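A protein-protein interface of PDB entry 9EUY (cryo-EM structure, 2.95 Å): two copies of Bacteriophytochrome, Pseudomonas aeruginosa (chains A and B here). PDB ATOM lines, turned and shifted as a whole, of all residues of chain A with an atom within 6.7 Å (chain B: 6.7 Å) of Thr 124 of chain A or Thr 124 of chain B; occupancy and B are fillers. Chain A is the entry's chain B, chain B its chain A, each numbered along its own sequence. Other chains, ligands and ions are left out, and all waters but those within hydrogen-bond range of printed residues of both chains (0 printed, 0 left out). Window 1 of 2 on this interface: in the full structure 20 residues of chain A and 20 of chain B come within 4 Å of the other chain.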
ATOM      1  N   SER A 119      29.425 -11.386   6.238  1.00  0.00           N
ATOM      2  CA  SER A 119      28.187 -10.926   5.628  1.00  0.00           C
ATOM      3  C   SER A 119      26.994 -11.620   6.263  1.00  0.00           C
ATOM      4  O   SER A 119      25.930 -11.018   6.415  1.00  0.00           O
ATOM      5  CB  SER A 119      28.218 -11.169   4.120  1.00  0.00           C
ATOM      6  OG  SER A 119      29.328 -10.518   3.527  1.00  0.00           O
ATOM      7  N   ILE A 120      27.144 -12.901   6.610  1.00  0.00           N
ATOM      8  CA  ILE A 120      26.050 -13.626   7.250  1.00  0.00           C
ATOM      9  C   ILE A 120      25.707 -12.996   8.593  1.00  0.00           C
ATOM     10  O   ILE A 120      24.529 -12.831   8.934  1.00  0.00           O
ATOM     11  CB  ILE A 120      26.415 -15.114   7.398  1.00  0.00           C
ATOM     12  CG1 ILE A 120      26.417 -15.794   6.031  1.00  0.00           C
ATOM     13  CG2 ILE A 120      25.449 -15.817   8.336  1.00  0.00           C
ATOM     14  CD1 ILE A 120      27.000 -17.175   6.044  1.00  0.00           C
ATOM     15  N   THR A 121      26.724 -12.579   9.350  1.00  0.00           N
ATOM     16  CA  THR A 121      26.474 -11.931  10.635  1.00  0.00           C
ATOM     17  C   THR A 121      25.785 -10.582  10.452  1.00  0.00           C
ATOM     18  O   THR A 121      24.816 -10.265  11.155  1.00  0.00           O
ATOM     19  CB  THR A 121      27.777 -11.770  11.416  1.00  0.00           C
ATOM     20  OG1 THR A 121      28.347 -13.060  11.658  1.00  0.00           O
ATOM     21  CG2 THR A 121      27.498 -11.120  12.752  1.00  0.00           C
ATOM     22  N   SER A 122      26.287  -9.763   9.525  1.00  0.00           N
ATOM     23  CA  SER A 122      25.663  -8.465   9.266  1.00  0.00           C
ATOM     24  C   SER A 122      24.223  -8.617   8.782  1.00  0.00           C
ATOM     25  O   SER A 122      23.329  -7.878   9.213  1.00  0.00           O
ATOM     26  CB  SER A 122      26.489  -7.682   8.248  1.00  0.00           C
ATOM     27  OG  SER A 122      27.764  -7.358   8.772  1.00  0.00           O
ATOM     28  N   PHE A 123      23.988  -9.561   7.871  1.00  0.00           N
ATOM     29  CA  PHE A 123      22.651  -9.814   7.345  1.00  0.00           C
ATOM     30  C   PHE A 123      21.722 -10.309   8.449  1.00  0.00           C
ATOM     31  O   PHE A 123      20.542  -9.935   8.503  1.00  0.00           O
ATOM     32  CB  PHE A 123      22.782 -10.835   6.213  1.00  0.00           C
ATOM     33  CG  PHE A 123      21.635 -10.864   5.244  1.00  0.00           C
ATOM     34  CD1 PHE A 123      20.481 -10.136   5.456  1.00  0.00           C
ATOM     35  CD2 PHE A 123      21.741 -11.618   4.087  1.00  0.00           C
ATOM     36  CE1 PHE A 123      19.449 -10.181   4.540  1.00  0.00           C
ATOM     37  CE2 PHE A 123      20.717 -11.662   3.175  1.00  0.00           C
ATOM     38  CZ  PHE A 123      19.570 -10.944   3.400  1.00  0.00           C
ATOM     39  N   THR A 124      22.259 -11.100   9.381  1.00  0.00           N
ATOM     40  CA  THR A 124      21.471 -11.561  10.517  1.00  0.00           C
ATOM     41  C   THR A 124      21.108 -10.401  11.432  1.00  0.00           C
ATOM     42  O   THR A 124      19.977 -10.325  11.926  1.00  0.00           O
ATOM     43  CB  THR A 124      22.239 -12.633  11.286  1.00  0.00           C
ATOM     44  OG1 THR A 124      22.454 -13.767  10.438  1.00  0.00           O
ATOM     45  CG2 THR A 124      21.458 -13.072  12.510  1.00  0.00           C
ATOM     46  N   LEU A 125      22.053  -9.489  11.670  1.00  0.00           N
ATOM     47  CA  LEU A 125      21.752  -8.310  12.478  1.00  0.00           C
ATOM     48  C   LEU A 125      20.677  -7.448  11.827  1.00  0.00           C
ATOM     49  O   LEU A 125      19.774  -6.953  12.511  1.00  0.00           O
ATOM     50  CB  LEU A 125      23.018  -7.484  12.713  1.00  0.00           C
ATOM     51  CG  LEU A 125      24.036  -7.975  13.739  1.00  0.00           C
ATOM     52  CD1 LEU A 125      25.312  -7.158  13.642  1.00  0.00           C
ATOM     53  CD2 LEU A 125      23.451  -7.888  15.136  1.00  0.00           C
ATOM     54  N   ASN A 126      20.767  -7.235  10.512  1.00  0.00           N
ATOM     55  CA  ASN A 126      19.736  -6.455   9.830  1.00  0.00           C
ATOM     56  C   ASN A 126      18.365  -7.117   9.950  1.00  0.00           C
ATOM     57  O   ASN A 126      17.357  -6.445  10.220  1.00  0.00           O
ATOM     58  CB  ASN A 126      20.107  -6.256   8.362  1.00  0.00           C
ATOM     59  CG  ASN A 126      21.293  -5.335   8.177  1.00  0.00           C
ATOM     60  OD1 ASN A 126      21.647  -4.570   9.072  1.00  0.00           O
ATOM     61  ND2 ASN A 126      21.908  -5.395   7.003  1.00  0.00           N
ATOM     62  N   ALA A 127      18.302  -8.437   9.744  1.00  0.00           N
ATOM     63  CA  ALA A 127      17.030  -9.139   9.894  1.00  0.00           C
ATOM     64  C   ALA A 127      16.491  -9.014  11.313  1.00  0.00           C
ATOM     65  O   ALA A 127      15.291  -8.783  11.518  1.00  0.00           O
ATOM     66  CB  ALA A 127      17.195 -10.608   9.510  1.00  0.00           C
ATOM     67  N   GLN A 128      17.365  -9.174  12.309  1.00  0.00           N
ATOM     68  CA  GLN A 128      16.951  -9.041  13.698  1.00  0.00           C
ATOM     69  C   GLN A 128      16.453  -7.636  14.008  1.00  0.00           C
ATOM     70  O   GLN A 128      15.515  -7.468  14.800  1.00  0.00           O
ATOM     71  CB  GLN A 128      18.123  -9.419  14.603  1.00  0.00           C
ATOM     72  CG  GLN A 128      18.357 -10.922  14.678  1.00  0.00           C
ATOM     73  CD  GLN A 128      19.585 -11.295  15.481  1.00  0.00           C
ATOM     74  OE1 GLN A 128      20.512 -10.500  15.628  1.00  0.00           O
ATOM     75  NE2 GLN A 128      19.602 -12.518  15.997  1.00  0.00           N
ATOM     76  N   ARG A 129      17.034  -6.615  13.372  1.00  0.00           N
ATOM     77  CA  ARG A 129      16.512  -5.265  13.554  1.00  0.00           C
ATOM     78  C   ARG A 129      15.160  -5.088  12.886  1.00  0.00           C
ATOM     79  O   ARG A 129      14.352  -4.278  13.351  1.00  0.00           O
ATOM     80  CB  ARG A 129      17.514  -4.222  13.081  1.00  0.00           C
ATOM     81  CG  ARG A 129      18.610  -4.087  14.096  1.00  0.00           C
ATOM     82  CD  ARG A 129      19.441  -2.846  13.951  1.00  0.00           C
ATOM     83  NE  ARG A 129      20.058  -2.558  15.238  1.00  0.00           N
ATOM     84  CZ  ARG A 129      21.195  -3.094  15.658  1.00  0.00           C
ATOM     85  NH1 ARG A 129      21.871  -3.951  14.912  1.00  0.00           N
ATOM     86  NH2 ARG A 129      21.651  -2.779  16.867  1.00  0.00           N
ATOM     87  N   ILE A 131      12.964  -7.518  12.853  1.00  0.00           N
ATOM     88  CA  ILE A 131      12.133  -8.198  13.844  1.00  0.00           C
ATOM     89  C   ILE A 131      11.817  -7.264  15.006  1.00  0.00           C
ATOM     90  O   ILE A 131      10.686  -7.225  15.506  1.00  0.00           O
ATOM     91  CB  ILE A 131      12.820  -9.487  14.329  1.00  0.00           C
ATOM     92  CG1 ILE A 131      13.184 -10.380  13.146  1.00  0.00           C
ATOM     93  CG2 ILE A 131      11.914 -10.237  15.286  1.00  0.00           C
ATOM     94  CD1 ILE A 131      14.054 -11.553  13.520  1.00  0.00           C
ATOM     95  N   MET A 154      17.771  -4.655   2.607  1.00  0.00           N
ATOM     96  CA  MET A 154      18.629  -5.694   3.170  1.00  0.00           C
ATOM     97  C   MET A 154      19.021  -6.753   2.149  1.00  0.00           C
ATOM     98  O   MET A 154      20.206  -6.947   1.858  1.00  0.00           O
ATOM     99  CB  MET A 154      17.942  -6.372   4.346  1.00  0.00           C
ATOM    100  CG  MET A 154      17.819  -5.556   5.581  1.00  0.00           C
ATOM    101  SD  MET A 154      16.871  -6.565   6.708  1.00  0.00           S
ATOM    102  CE  MET A 154      17.720  -8.126   6.559  1.00  0.00           C
ATOM    103  N   PRO A 287      21.383 -19.368   7.892  1.00  0.00           N
ATOM    104  CA  PRO A 287      21.149 -18.605   9.133  1.00  0.00           C
ATOM    105  C   PRO A 287      20.283 -17.375   8.918  1.00  0.00           C
ATOM    106  O   PRO A 287      19.429 -17.048   9.757  1.00  0.00           O
ATOM    107  CB  PRO A 287      22.566 -18.226   9.582  1.00  0.00           C
ATOM    108  CG  PRO A 287      23.444 -19.247   8.962  1.00  0.00           C
ATOM    109  CD  PRO A 287      22.822 -19.556   7.641  1.00  0.00           C
ATOM    110  N   VAL A 288      20.412 -16.741   7.756  1.00  0.00           N
ATOM    111  CA  VAL A 288      19.594 -15.579   7.442  1.00  0.00           C
ATOM    112  C   VAL A 288      18.162 -16.006   7.166  1.00  0.00           C
ATOM    113  O   VAL A 288      17.212 -15.324   7.564  1.00  0.00           O
ATOM    114  CB  VAL A 288      20.200 -14.808   6.260  1.00  0.00           C
ATOM    115  CG1 VAL A 288      19.462 -13.513   6.053  1.00  0.00           C
ATOM    116  CG2 VAL A 288      21.669 -14.552   6.506  1.00  0.00           C
ATOM    117  N   MET A 290      16.736 -18.540   8.542  1.00  0.00           N
ATOM    118  CA  MET A 290      16.190 -18.816   9.870  1.00  0.00           C
ATOM    119  C   MET A 290      15.809 -17.527  10.597  1.00  0.00           C
ATOM    120  O   MET A 290      14.790 -17.478  11.307  1.00  0.00           O
ATOM    121  CB  MET A 290      17.204 -19.618  10.686  1.00  0.00           C
ATOM    122  CG  MET A 290      16.833 -19.812  12.143  1.00  0.00           C
ATOM    123  SD  MET A 290      15.194 -20.519  12.378  1.00  0.00           S
ATOM    124  CE  MET A 290      15.404 -22.094  11.555  1.00  0.00           C
ATOM    125  N   SER A 291      16.569 -16.454  10.369  1.00  0.00           N
ATOM    126  CA  SER A 291      16.215 -15.167  10.961  1.00  0.00           C
ATOM    127  C   SER A 291      14.938 -14.622  10.338  1.00  0.00           C
ATOM    128  O   SER A 291      14.084 -14.065  11.036  1.00  0.00           O
ATOM    129  CB  SER A 291      17.361 -14.171  10.800  1.00  0.00           C
ATOM    130  OG  SER A 291      18.568 -14.694  11.319  1.00  0.00           O
ATOM    131  N   ILE A 294      12.020 -16.430  11.877  1.00  0.00           N
ATOM    132  CA  ILE A 294      11.584 -15.838  13.136  1.00  0.00           C
ATOM    133  C   ILE A 294      10.863 -14.529  12.858  1.00  0.00           C
ATOM    134  O   ILE A 294       9.903 -14.172  13.549  1.00  0.00           O
ATOM    135  CB  ILE A 294      12.770 -15.646  14.093  1.00  0.00           C
ATOM    136  CG1 ILE A 294      13.303 -17.001  14.532  1.00  0.00           C
ATOM    137  CG2 ILE A 294      12.355 -14.847  15.310  1.00  0.00           C
ATOM    138  CD1 ILE A 294      14.623 -16.903  15.183  1.00  0.00           C
ATOM    139  N   SER B 119      31.310 -19.908  15.466  1.00  0.00           N
ATOM    140  CA  SER B 119      30.930 -19.963  16.877  1.00  0.00           C
ATOM    141  C   SER B 119      29.844 -18.927  17.134  1.00  0.00           C
ATOM    142  O   SER B 119      28.825 -19.252  17.742  1.00  0.00           O
ATOM    143  CB  SER B 119      32.124 -19.772  17.820  1.00  0.00           C
ATOM    144  OG  SER B 119      33.167 -20.681  17.511  1.00  0.00           O
ATOM    145  N   ILE B 120      30.042 -17.679  16.700  1.00  0.00           N
ATOM    146  CA  ILE B 120      28.976 -16.688  16.833  1.00  0.00           C
ATOM    147  C   ILE B 120      27.769 -17.098  16.000  1.00  0.00           C
ATOM    148  O   ILE B 120      26.626 -17.008  16.457  1.00  0.00           O
ATOM    149  CB  ILE B 120      29.469 -15.277  16.456  1.00  0.00           C
ATOM    150  CG1 ILE B 120      30.378 -14.720  17.550  1.00  0.00           C
ATOM    151  CG2 ILE B 120      28.295 -14.341  16.219  1.00  0.00           C
ATOM    152  CD1 ILE B 120      30.839 -13.301  17.295  1.00  0.00           C
ATOM    153  N   THR B 121      27.998 -17.550  14.764  1.00  0.00           N
ATOM    154  CA  THR B 121      26.884 -18.010  13.937  1.00  0.00           C
ATOM    155  C   THR B 121      26.166 -19.197  14.577  1.00  0.00           C
ATOM    156  O   THR B 121      24.932 -19.252  14.588  1.00  0.00           O
ATOM    157  CB  THR B 121      27.380 -18.375  12.539  1.00  0.00           C
ATOM    158  OG1 THR B 121      27.930 -17.212  11.909  1.00  0.00           O
ATOM    159  CG2 THR B 121      26.233 -18.897  11.693  1.00  0.00           C
ATOM    160  N   SER B 122      26.924 -20.148  15.128  1.00  0.00           N
ATOM    161  CA  SER B 122      26.333 -21.314  15.786  1.00  0.00           C
ATOM    162  C   SER B 122      25.560 -20.926  17.044  1.00  0.00           C
ATOM    163  O   SER B 122      24.477 -21.463  17.307  1.00  0.00           O
ATOM    164  CB  SER B 122      27.425 -22.330  16.117  1.00  0.00           C
ATOM    165  OG  SER B 122      28.189 -22.641  14.967  1.00  0.00           O
ATOM    166  N   PHE B 123      26.094 -19.988  17.824  1.00  0.00           N
ATOM    167  CA  PHE B 123      25.436 -19.519  19.039  1.00  0.00           C
ATOM    168  C   PHE B 123      24.158 -18.762  18.691  1.00  0.00           C
ATOM    169  O   PHE B 123      23.127 -18.916  19.360  1.00  0.00           O
ATOM    170  CB  PHE B 123      26.431 -18.636  19.797  1.00  0.00           C
ATOM    171  CG  PHE B 123      26.088 -18.370  21.236  1.00  0.00           C
ATOM    172  CD1 PHE B 123      24.904 -18.800  21.802  1.00  0.00           C
ATOM    173  CD2 PHE B 123      26.991 -17.687  22.031  1.00  0.00           C
ATOM    174  CE1 PHE B 123      24.628 -18.542  23.130  1.00  0.00           C
ATOM    175  CE2 PHE B 123      26.719 -17.429  23.352  1.00  0.00           C
ATOM    176  CZ  PHE B 123      25.537 -17.856  23.903  1.00  0.00           C
ATOM    177  N   THR B 124      24.195 -17.988  17.607  1.00  0.00           N
ATOM    178  CA  THR B 124      23.006 -17.285  17.148  1.00  0.00           C
ATOM    179  C   THR B 124      21.955 -18.276  16.671  1.00  0.00           C
ATOM    180  O   THR B 124      20.765 -18.106  16.952  1.00  0.00           O
ATOM    181  CB  THR B 124      23.367 -16.300  16.039  1.00  0.00           C
ATOM    182  OG1 THR B 124      24.305 -15.343  16.539  1.00  0.00           O
ATOM    183  CG2 THR B 124      22.130 -15.568  15.562  1.00  0.00           C
ATOM    184  N   LEU B 125      22.375 -19.304  15.927  1.00  0.00           N
ATOM    185  CA  LEU B 125      21.444 -20.341  15.496  1.00  0.00           C
ATOM    186  C   LEU B 125      20.801 -21.040  16.687  1.00  0.00           C
ATOM    187  O   LEU B 125      19.602 -21.327  16.667  1.00  0.00           O
ATOM    188  CB  LEU B 125      22.158 -21.357  14.605  1.00  0.00           C
ATOM    189  CG  LEU B 125      22.369 -20.999  13.134  1.00  0.00           C
ATOM    190  CD1 LEU B 125      23.299 -22.001  12.468  1.00  0.00           C
ATOM    191  CD2 LEU B 125      21.036 -20.947  12.414  1.00  0.00           C
ATOM    192  N   ASN B 126      21.591 -21.370  17.710  1.00  0.00           N
ATOM    193  CA  ASN B 126      21.031 -21.989  18.911  1.00  0.00           C
ATOM    194  C   ASN B 126      19.997 -21.081  19.577  1.00  0.00           C
ATOM    195  O   ASN B 126      18.913 -21.534  19.977  1.00  0.00           O
ATOM    196  CB  ASN B 126      22.152 -22.340  19.885  1.00  0.00           C
ATOM    197  CG  ASN B 126      22.669 -23.745  19.692  1.00  0.00           C
ATOM    198  OD1 ASN B 126      22.148 -24.694  20.275  1.00  0.00           O
ATOM    199  ND2 ASN B 126      23.699 -23.889  18.868  1.00  0.00           N
ATOM    200  N   ALA B 127      20.319 -19.790  19.711  1.00  0.00           N
ATOM    201  CA  ALA B 127      19.363 -18.852  20.293  1.00  0.00           C
ATOM    202  C   ALA B 127      18.092 -18.777  19.457  1.00  0.00           C
ATOM    203  O   ALA B 127      16.980 -18.735  19.994  1.00  0.00           O
ATOM    204  CB  ALA B 127      19.999 -17.471  20.426  1.00  0.00           C
ATOM    205  N   GLN B 128      18.246 -18.763  18.135  1.00  0.00           N
ATOM    206  CA  GLN B 128      17.104 -18.740  17.235  1.00  0.00           C
ATOM    207  C   GLN B 128      16.272 -20.011  17.353  1.00  0.00           C
ATOM    208  O   GLN B 128      15.041 -19.963  17.240  1.00  0.00           O
ATOM    209  CB  GLN B 128      17.607 -18.528  15.810  1.00  0.00           C
ATOM    210  CG  GLN B 128      18.110 -17.110  15.585  1.00  0.00           C
ATOM    211  CD  GLN B 128      18.691 -16.895  14.210  1.00  0.00           C
ATOM    212  OE1 GLN B 128      18.918 -17.843  13.463  1.00  0.00           O
ATOM    213  NE2 GLN B 128      18.939 -15.639  13.865  1.00  0.00           N
ATOM    214  N   ARG B 129      16.922 -21.151  17.593  1.00  0.00           N
ATOM    215  CA  ARG B 129      16.183 -22.385  17.828  1.00  0.00           C
ATOM    216  C   ARG B 129      15.359 -22.273  19.100  1.00  0.00           C
ATOM    217  O   ARG B 129      14.212 -22.732  19.145  1.00  0.00           O
ATOM    218  CB  ARG B 129      17.133 -23.578  17.903  1.00  0.00           C
ATOM    219  CG  ARG B 129      17.730 -23.978  16.570  1.00  0.00           C
ATOM    220  CD  ARG B 129      18.711 -25.118  16.742  1.00  0.00           C
ATOM    221  NE  ARG B 129      19.793 -25.052  15.768  1.00  0.00           N
ATOM    222  CZ  ARG B 129      21.078 -25.173  16.073  1.00  0.00           C
ATOM    223  NH1 ARG B 129      21.472 -25.460  17.303  1.00  0.00           N
ATOM    224  NH2 ARG B 129      21.988 -25.027  15.115  1.00  0.00           N
ATOM    225  N   ILE B 131      14.164 -19.492  20.311  1.00  0.00           N
ATOM    226  CA  ILE B 131      13.075 -18.580  19.963  1.00  0.00           C
ATOM    227  C   ILE B 131      11.963 -19.328  19.237  1.00  0.00           C
ATOM    228  O   ILE B 131      10.773 -19.086  19.473  1.00  0.00           O
ATOM    229  CB  ILE B 131      13.605 -17.402  19.126  1.00  0.00           C
ATOM    230  CG1 ILE B 131      14.654 -16.618  19.908  1.00  0.00           C
ATOM    231  CG2 ILE B 131      12.469 -16.478  18.734  1.00  0.00           C
ATOM    232  CD1 ILE B 131      15.457 -15.663  19.058  1.00  0.00           C
ATOM    233  N   MET B 154      23.291 -23.773  26.067  1.00  0.00           N
ATOM    234  CA  MET B 154      23.897 -22.913  25.050  1.00  0.00           C
ATOM    235  C   MET B 154      24.986 -22.013  25.614  1.00  0.00           C
ATOM    236  O   MET B 154      26.120 -22.013  25.125  1.00  0.00           O
ATOM    237  CB  MET B 154      22.843 -22.042  24.387  1.00  0.00           C
ATOM    238  CG  MET B 154      21.835 -22.747  23.553  1.00  0.00           C
ATOM    239  SD  MET B 154      20.628 -21.492  23.148  1.00  0.00           S
ATOM    240  CE  MET B 154      21.697 -20.158  22.634  1.00  0.00           C
ATOM    241  N   PRO B 287      25.784  -9.707  18.742  1.00  0.00           N
ATOM    242  CA  PRO B 287      24.741 -10.362  17.931  1.00  0.00           C
ATOM    243  C   PRO B 287      23.958 -11.410  18.701  1.00  0.00           C
ATOM    244  O   PRO B 287      22.734 -11.528  18.540  1.00  0.00           O
ATOM    245  CB  PRO B 287      25.536 -10.986  16.776  1.00  0.00           C
ATOM    246  CG  PRO B 287      26.759 -10.162  16.675  1.00  0.00           C
ATOM    247  CD  PRO B 287      27.097  -9.767  18.079  1.00  0.00           C
ATOM    248  N   VAL B 288      24.624 -12.114  19.613  1.00  0.00           N
ATOM    249  CA  VAL B 288      23.950 -13.107  20.436  1.00  0.00           C
ATOM    250  C   VAL B 288      23.036 -12.422  21.442  1.00  0.00           C
ATOM    251  O   VAL B 288      21.925 -12.893  21.714  1.00  0.00           O
ATOM    252  CB  VAL B 288      24.984 -14.017  21.118  1.00  0.00           C
ATOM    253  CG1 VAL B 288      24.295 -15.064  21.954  1.00  0.00           C
ATOM    254  CG2 VAL B 288      25.869 -14.668  20.077  1.00  0.00           C
ATOM    255  N   MET B 290      21.560  -9.567  20.973  1.00  0.00           N
ATOM    256  CA  MET B 290      20.404  -9.123  20.196  1.00  0.00           C
ATOM    257  C   MET B 290      19.454 -10.282  19.904  1.00  0.00           C
ATOM    258  O   MET B 290      18.223 -10.111  19.923  1.00  0.00           O
ATOM    259  CB  MET B 290      20.877  -8.468  18.898  1.00  0.00           C
ATOM    260  CG  MET B 290      19.780  -8.193  17.886  1.00  0.00           C
ATOM    261  SD  MET B 290      18.406  -7.233  18.549  1.00  0.00           S
ATOM    262  CE  MET B 290      19.262  -5.747  19.061  1.00  0.00           C
ATOM    263  N   SER B 291      20.007 -11.483  19.723  1.00  0.00           N
ATOM    264  CA  SER B 291      19.163 -12.663  19.565  1.00  0.00           C
ATOM    265  C   SER B 291      18.384 -12.933  20.843  1.00  0.00           C
ATOM    266  O   SER B 291      17.191 -13.250  20.798  1.00  0.00           O
ATOM    267  CB  SER B 291      20.009 -13.875  19.183  1.00  0.00           C
ATOM    268  OG  SER B 291      20.778 -13.613  18.025  1.00  0.00           O
ATOM    269  N   ILE B 294      15.485 -10.507  21.168  1.00  0.00           N
ATOM    270  CA  ILE B 294      14.299 -10.945  20.441  1.00  0.00           C
ATOM    271  C   ILE B 294      13.659 -12.103  21.184  1.00  0.00           C
ATOM    272  O   ILE B 294      12.430 -12.239  21.217  1.00  0.00           O
ATOM    273  CB  ILE B 294      14.653 -11.317  18.994  1.00  0.00           C
ATOM    274  CG1 ILE B 294      15.072 -10.071  18.231  1.00  0.00           C
ATOM    275  CG2 ILE B 294      13.469 -11.960  18.300  1.00  0.00           C
ATOM    276  CD1 ILE B 294      15.811 -10.387  16.998  1.00  0.00           C
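The side-chain hydroxyl (OG) of Ser 291 of chain A lies within hydrogen-bond range of the side-chain amide nitrogen (NE2) of Gln 128 of chain B (2.7 Å).
The side-chain hydroxyl (OG) of Ser 291 of chain B sits at hydrogen-bond distance from the side-chain amide nitrogen (NE2) of Gln 128 of chain A, at 2.6 Å.
The backbone carbonyl oxygen (O) of Ile 120 of chain B lies within hydrogen-bond range of the side-chain hydroxyl (OG1) of Thr 124 of chain B.
O of Pro 287 of chain B sits at hydrogen-bond distance from OG of Ser 291 of chain B, at 2.9 Å.
The side-chain hydroxyl (OG1) of Thr 124 of chain A is in hydrogen-bond range of the backbone carbonyl oxygen (O) of Ile 120 of chain A (2.7 Å).
The backbone carbonyl oxygen (O) of Pro 287 of chain A sits at hydrogen-bond distance from the side-chain hydroxyl (OG) of Ser 291 of chain A.
Among the printed residues, merely in contact across the chains: Thr 124 of chain A with Thr 124 of chain B (3.9995 Å), Thr 124 of chain A with Gln 128 of chain B (3.8 Å), Leu 125 of chain A with Pro 287 of chain B (3.9 Å), Gln 128 of chain A with Thr 124 of chain B (3.99 Å), Gln 128 of chain A with Gln 128 of chain B (3.8 Å), Gln 128 of chain A with Pro 287 of chain B (3.8 Å), Gln 128 of chain A with Met 290 of chain B (3.3 Å), Gln 128 of chain A with Ile 294 of chain B (3.5 Å), Ile 131 of chain A with Ile 294 of chain B (3.8 Å), Pro 287 of chain A with Thr 121 of chain B (3.9 Å), Pro 287 of chain A with Gln 128 of chain B (3.8 Å), Met 290 of chain A with Gln 128 of chain B (3.2 Å), Ile 294 of chain A with Gln 128 of chain B (3.5 Å) and Ile 294 of chain A with Ile 131 of chain B (3.8 Å).
Of the printed residues of chain B, Thr 124 of chain A touches Thr 124 and Gln 128.
Of the printed residues of chain B, Leu 125 of chain A touches Pro 287.
Of the printed residues of chain B, Gln 128 of chain A touches Thr 124 (3.99 Å), Gln 128 (3.8 Å), Pro 287 (3.8 Å), Met 290 (3.3 Å), Ser 291 (2.6 Å) and Ile 294 (3.5 Å).
Of the printed residues of chain B, Ile 294 of chain A touches Gln 128 and Ile 131.
Ser 119 of chain B touches none of the printed residues of chain A.
The nearest printed residue of chain B that does not touch Thr 124 of chain A is Ser 291 of chain B (5.6 Å).
The nearest printed residue of chain A that does not touch Thr 124 of chain B is Ser 291 of chain A (5.6 Å).
The nearest printed residue of chain A that does not touch Gln 128 of chain B is Val 288 of chain A (6.0 Å).
Thr 124 of chain B touches its own counterpart, Thr 124 of chain A.
Thr 124 of chain A touches Gln 128 of chain B, and with the chains exchanged Gln 128 of chain A touches Thr 124 of chain B.
Gln 128 of chain A touches Ile 294 of chain B, and with the chains exchanged Ile 294 of chain A touches Gln 128 of chain B.
Pro 287 of chain A touches Thr 121 of chain B, but with the chains exchanged Thr 121 of chain A does not touch Pro 287 of chain B (4.1 Å).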
